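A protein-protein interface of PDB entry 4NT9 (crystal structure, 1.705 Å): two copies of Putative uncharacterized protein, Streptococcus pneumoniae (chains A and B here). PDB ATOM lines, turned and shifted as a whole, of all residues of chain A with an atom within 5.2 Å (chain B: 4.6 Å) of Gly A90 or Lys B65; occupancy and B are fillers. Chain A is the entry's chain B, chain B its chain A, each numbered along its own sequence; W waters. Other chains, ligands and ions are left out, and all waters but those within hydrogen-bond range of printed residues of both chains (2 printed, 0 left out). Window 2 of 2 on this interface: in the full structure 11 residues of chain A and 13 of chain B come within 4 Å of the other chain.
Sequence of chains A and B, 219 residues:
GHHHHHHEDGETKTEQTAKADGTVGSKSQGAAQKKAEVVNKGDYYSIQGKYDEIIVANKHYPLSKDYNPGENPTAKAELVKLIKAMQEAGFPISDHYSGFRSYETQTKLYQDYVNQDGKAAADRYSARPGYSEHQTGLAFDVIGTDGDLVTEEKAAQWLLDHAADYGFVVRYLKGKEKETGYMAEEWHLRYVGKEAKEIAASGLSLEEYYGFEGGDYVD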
ATOM      1  N   MET A  86      12.720  19.282 -10.213  1.00  0.00           N
ATOM      2  CA  MET A  86      12.655  17.903 -10.707  1.00  0.00           C
ATOM      3  C   MET A  86      13.363  16.952  -9.751  1.00  0.00           C
ATOM      4  O   MET A  86      12.899  15.847  -9.519  1.00  0.00           O
ATOM      5  CB  MET A  86      13.359  17.757 -12.060  1.00  0.00           C
ATOM      6  CG  MET A  86      12.627  18.331 -13.206  1.00  0.00           C
ATOM      7  SD  MET A  86      13.241  17.725 -14.809  1.00  0.00           S
ATOM      8  CE  MET A  86      12.525  16.099 -14.828  1.00  0.00           C
ATOM      9  N   GLN A  87      14.520  17.367  -9.253  1.00  0.00           N
ATOM     10  CA  GLN A  87      15.257  16.534  -8.317  1.00  0.00           C
ATOM     11  C   GLN A  87      14.426  16.312  -7.056  1.00  0.00           C
ATOM     12  O   GLN A  87      14.400  15.204  -6.529  1.00  0.00           O
ATOM     13  CB  GLN A  87      16.594  17.176  -7.972  1.00  0.00           C
ATOM     14  CG  GLN A  87      17.517  17.305  -9.177  1.00  0.00           C
ATOM     15  CD  GLN A  87      18.695  18.232  -8.922  1.00  0.00           C
ATOM     16  OE1 GLN A  87      18.640  19.088  -8.042  1.00  0.00           O
ATOM     17  NE2 GLN A  87      19.784  18.046  -9.680  1.00  0.00           N
ATOM     18  N   GLU A  88      13.760  17.359  -6.561  1.00  0.00           N
ATOM     19  CA  GLU A  88      12.894  17.195  -5.369  1.00  0.00           C
ATOM     20  C   GLU A  88      11.724  16.273  -5.646  1.00  0.00           C
ATOM     21  O   GLU A  88      11.186  15.631  -4.726  1.00  0.00           O
ATOM     22  CB  GLU A  88      12.409  18.537  -4.836  1.00  0.00           C
ATOM     23  CG  GLU A  88      13.569  19.358  -4.299  1.00  0.00           C
ATOM     24  CD  GLU A  88      13.228  20.790  -4.074  1.00  0.00           C
ATOM     25  OE1 GLU A  88      12.142  21.238  -4.517  1.00  0.00           O
ATOM     26  OE2 GLU A  88      14.078  21.480  -3.478  1.00  0.00           O
ATOM     27  N   ALA A  89      11.334  16.185  -6.910  1.00  0.00           N
ATOM     28  CA  ALA A  89      10.216  15.316  -7.260  1.00  0.00           C
ATOM     29  C   ALA A  89      10.679  13.873  -7.402  1.00  0.00           C
ATOM     30  O   ALA A  89       9.887  12.989  -7.754  1.00  0.00           O
ATOM     31  CB  ALA A  89       9.533  15.784  -8.523  1.00  0.00           C
ATOM     32  N   GLY A  90      11.962  13.636  -7.147  1.00  0.00           N
ATOM     33  CA  GLY A  90      12.504  12.292  -7.200  1.00  0.00           C
ATOM     34  C   GLY A  90      13.175  11.865  -8.497  1.00  0.00           C
ATOM     35  O   GLY A  90      13.579  10.704  -8.628  1.00  0.00           O
ATOM     36  N   PHE A  91      13.321  12.775  -9.465  1.00  0.00           N
ATOM     37  CA  PHE A  91      13.950  12.376 -10.716  1.00  0.00           C
ATOM     38  C   PHE A  91      15.449  12.595 -10.630  1.00  0.00           C
ATOM     39  O   PHE A  91      15.908  13.600 -10.089  1.00  0.00           O
ATOM     40  CB  PHE A  91      13.339  13.131 -11.908  1.00  0.00           C
ATOM     41  CG  PHE A  91      11.856  12.892 -12.081  1.00  0.00           C
ATOM     42  CD1 PHE A  91      11.399  11.777 -12.766  1.00  0.00           C
ATOM     43  CD2 PHE A  91      10.931  13.787 -11.548  1.00  0.00           C
ATOM     44  CE1 PHE A  91      10.039  11.545 -12.919  1.00  0.00           C
ATOM     45  CE2 PHE A  91       9.570  13.578 -11.696  1.00  0.00           C
ATOM     46  CZ  PHE A  91       9.121  12.446 -12.392  1.00  0.00           C
ATOM     47  N   PRO A  92      16.224  11.651 -11.187  1.00  0.00           N
ATOM     48  CA  PRO A  92      17.685  11.678 -11.145  1.00  0.00           C
ATOM     49  C   PRO A  92      18.232  12.589 -12.252  1.00  0.00           C
ATOM     50  O   PRO A  92      18.864  12.132 -13.220  1.00  0.00           O
ATOM     51  CB  PRO A  92      18.052  10.213 -11.430  1.00  0.00           C
ATOM     52  CG  PRO A  92      16.988   9.761 -12.382  1.00  0.00           C
ATOM     53  CD  PRO A  92      15.714  10.444 -11.851  1.00  0.00           C
ATOM     54  N   GLU A 152      13.147   9.162 -20.021  1.00  0.00           N
ATOM     55  CA  GLU A 152      12.226   8.353 -19.212  1.00  0.00           C
ATOM     56  C   GLU A 152      10.816   8.974 -19.152  1.00  0.00           C
ATOM     57  O   GLU A 152      10.654  10.187 -19.030  1.00  0.00           O
ATOM     58  CB  GLU A 152      12.771   8.138 -17.802  1.00  0.00           C
ATOM     59  CG  GLU A 152      11.971   7.082 -17.001  1.00  0.00           C
ATOM     60  CD  GLU A 152      10.744   7.665 -16.302  1.00  0.00           C
ATOM     61  OE1 GLU A 152      10.845   8.814 -15.863  1.00  0.00           O
ATOM     62  OE2 GLU A 152       9.682   6.991 -16.193  1.00  0.00           O
ATOM     63  N   LYS A 154       8.011   9.180 -17.205  1.00  0.00           N
ATOM     64  CA  LYS A 154       7.493  10.052 -16.138  1.00  0.00           C
ATOM     65  C   LYS A 154       8.254  11.369 -16.061  1.00  0.00           C
ATOM     66  O   LYS A 154       7.657  12.427 -15.826  1.00  0.00           O
ATOM     67  CB  LYS A 154       7.577   9.351 -14.800  1.00  0.00           C
ATOM     68  CG  LYS A 154       6.538   8.229 -14.681  1.00  0.00           C
ATOM     69  CD  LYS A 154       6.786   7.422 -13.433  1.00  0.00           C
ATOM     70  CE  LYS A 154       5.635   6.470 -13.173  1.00  0.00           C
ATOM     71  NZ  LYS A 154       5.519   5.417 -14.233  1.00  0.00           N
ATOM     72  N   LEU B  63       5.568  13.678  -3.539  1.00  0.00           N
ATOM     73  CA  LEU B  63       5.955  12.292  -3.344  1.00  0.00           C
ATOM     74  C   LEU B  63       6.702  11.799  -4.563  1.00  0.00           C
ATOM     75  O   LEU B  63       6.369  12.160  -5.677  1.00  0.00           O
ATOM     76  CB  LEU B  63       4.714  11.438  -3.127  1.00  0.00           C
ATOM     77  CG  LEU B  63       3.939  11.985  -1.928  1.00  0.00           C
ATOM     78  CD1 LEU B  63       2.523  11.467  -1.895  1.00  0.00           C
ATOM     79  CD2 LEU B  63       4.632  11.603  -0.635  1.00  0.00           C
ATOM     80  N   SER B  64       7.702  10.962  -4.341  1.00  0.00           N
ATOM     81  CA  SER B  64       8.420  10.309  -5.424  1.00  0.00           C
ATOM     82  C   SER B  64       7.493   9.539  -6.365  1.00  0.00           C
ATOM     83  O   SER B  64       6.449   8.994  -5.938  1.00  0.00           O
ATOM     84  CB  SER B  64       9.438   9.323  -4.843  1.00  0.00           C
ATOM     85  OG  SER B  64       9.820   8.377  -5.829  1.00  0.00           O
ATOM     86  N   LYS B  65       7.890   9.445  -7.628  1.00  0.00           N
ATOM     87  CA  LYS B  65       7.152   8.633  -8.585  1.00  0.00           C
ATOM     88  C   LYS B  65       7.132   7.164  -8.186  1.00  0.00           C
ATOM     89  O   LYS B  65       6.329   6.375  -8.708  1.00  0.00           O
ATOM     90  CB  LYS B  65       7.750   8.771  -9.993  1.00  0.00           C
ATOM     91  CG  LYS B  65       9.234   8.375 -10.057  1.00  0.00           C
ATOM     92  CD  LYS B  65       9.647   7.828 -11.411  1.00  0.00           C
ATOM     93  CE  LYS B  65      11.105   7.369 -11.358  1.00  0.00           C
ATOM     94  NZ  LYS B  65      11.892   8.429 -10.680  1.00  0.00           N
ATOM     95  N   ASP B  66       8.011   6.792  -7.263  1.00  0.00           N
ATOM     96  CA  ASP B  66       8.165   5.385  -6.893  1.00  0.00           C
ATOM     97  C   ASP B  66       7.496   5.090  -5.564  1.00  0.00           C
ATOM     98  O   ASP B  66       7.411   3.928  -5.140  1.00  0.00           O
ATOM     99  CB  ASP B  66       9.651   5.003  -6.822  1.00  0.00           C
ATOM    100  CG  ASP B  66      10.339   5.087  -8.176  1.00  0.00           C
ATOM    101  OD1 ASP B  66       9.729   4.638  -9.170  1.00  0.00           O
ATOM    102  OD2 ASP B  66      11.471   5.621  -8.248  1.00  0.00           O
ATOM    103  N   TYR B  67       6.999   6.139  -4.904  1.00  0.00           N
ATOM    104  CA  TYR B  67       6.370   5.952  -3.594  1.00  0.00           C
ATOM    105  C   TYR B  67       4.966   5.378  -3.763  1.00  0.00           C
ATOM    106  O   TYR B  67       4.075   6.040  -4.308  1.00  0.00           O
ATOM    107  CB  TYR B  67       6.304   7.274  -2.829  1.00  0.00           C
ATOM    108  CG  TYR B  67       5.814   7.101  -1.398  1.00  0.00           C
ATOM    109  CD1 TYR B  67       6.446   6.209  -0.528  1.00  0.00           C
ATOM    110  CD2 TYR B  67       4.723   7.818  -0.923  1.00  0.00           C
ATOM    111  CE1 TYR B  67       6.012   6.040   0.782  1.00  0.00           C
ATOM    112  CE2 TYR B  67       4.270   7.659   0.401  1.00  0.00           C
ATOM    113  CZ  TYR B  67       4.922   6.772   1.243  1.00  0.00           C
ATOM    114  OH  TYR B  67       4.493   6.611   2.550  1.00  0.00           O
ATOM    115  N   TYR B 103       0.823   7.048  -8.110  1.00  0.00           N
ATOM    116  CA  TYR B 103       1.348   8.025  -9.060  1.00  0.00           C
ATOM    117  C   TYR B 103       0.722   7.787 -10.418  1.00  0.00           C
ATOM    118  O   TYR B 103       0.303   8.740 -11.088  1.00  0.00           O
ATOM    119  CB  TYR B 103       2.854   7.881  -9.132  1.00  0.00           C
ATOM    120  CG  TYR B 103       3.586   9.004  -9.852  1.00  0.00           C
ATOM    121  CD1 TYR B 103       4.062  10.111  -9.150  1.00  0.00           C
ATOM    122  CD2 TYR B 103       3.838   8.911 -11.204  1.00  0.00           C
ATOM    123  CE1 TYR B 103       4.741  11.138  -9.805  1.00  0.00           C
ATOM    124  CE2 TYR B 103       4.512   9.925 -11.880  1.00  0.00           C
ATOM    125  CZ  TYR B 103       4.978  11.014 -11.161  1.00  0.00           C
ATOM    126  OH  TYR B 103       5.649  12.028 -11.819  1.00  0.00           O
ATOM    127  N   GLU B 104       0.653   6.508 -10.817  1.00  0.00           N
ATOM    128  CA  GLU B 104       0.109   6.132 -12.099  1.00  0.00           C
ATOM    129  C   GLU B 104      -1.357   6.473 -12.226  1.00  0.00           C
ATOM    130  O   GLU B 104      -1.786   6.926 -13.280  1.00  0.00           O
ATOM    131  CB  GLU B 104       0.356   4.633 -12.384  1.00  0.00           C
ATOM    132  CG  GLU B 104       1.841   4.273 -12.591  1.00  0.00           C
ATOM    133  CD  GLU B 104       2.673   4.273 -11.297  1.00  0.00           C
ATOM    134  OE1 GLU B 104       2.107   4.181 -10.154  1.00  0.00           O
ATOM    135  OE2 GLU B 104       3.921   4.361 -11.435  1.00  0.00           O
HETATM  136  O   HOH W   1       5.259  12.524 -14.396  1.00  0.00           O
HETATM  137  O   HOH W   2       7.173  13.166  -7.935  1.00  0.00           O
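Printed residues of chain B within 4 Å of Gly A90: Lys B65.
Printed residues of chain B within 4 Å of Phe A91: Lys B65 and Tyr B103.
Of the printed residues of chain B, Ala A89 touches Ser B64 (3.8 Å).
Of the printed residues of chain A, Ser B64 touches Ala A89 (3.8 Å).
Printed residues of chain B within 4 Å of Lys A154: Lys B65 (3.5 Å), Tyr B103 (3.6 Å) and Glu B104 (3.2 Å).
The nearest residue of chain A that does not touch Lys B65 is Ala A89 (4.1 Å).
No position is printed for both chains.
Of the 7 pairs that touch across the chains among the printed residues, none has its exchanged pair printed and touching as well.
Hydrophobic or aromatic side chains of chain B within 4 Å of the printed part of chain A: Tyr B103.
Of the 9 printed residues of chain A, 4 touch a printed residue of chain B.
Among the printed residues, Asp or Glu carboxylates within 4 Å of a Lys or Arg side-chain nitrogen of the other chain: Lys A154 with Glu B104.
The backbone NH (N) of Asp B66 sits at hydrogen-bond distance from the side-chain hydroxyl (OG) of Ser B64 (2.8 Å).
O of Met A86 sits at hydrogen-bond distance from N of Phe A91, at 3.1 Å.
The backbone NH (N) of Lys A154 lies within hydrogen-bond range of the side-chain carboxylate (OE2) of Glu A152 (2.9 Å).
NZ of Lys B65 is in salt-bridge range of OD2 of Asp B66 (3.7 Å).
Among the printed residues, merely in contact across the chains: Ala A89 with Ser B64, Phe A91 with Lys B65, Phe A91 with Tyr B103, Lys A154 with Lys B65 and Lys A154 with Tyr B103.
NZ of Lys A154 is in salt-bridge range of OE2 of Glu B104, 3.4 Å away.
The backbone carbonyl oxygen (O) of Gly A90 is in hydrogen-bond range of the side-chain amino group (NZ) of Lys B65.
Water W2 bridges O of Leu B63 (2.6 Å) and O of Ala A89 (2.7 Å).
Water W1 bridges the side-chain hydroxyl (OH) of Tyr B103 (2.7 Å) and the backbone carbonyl oxygen (O) of Lys A154 (2.8 Å).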
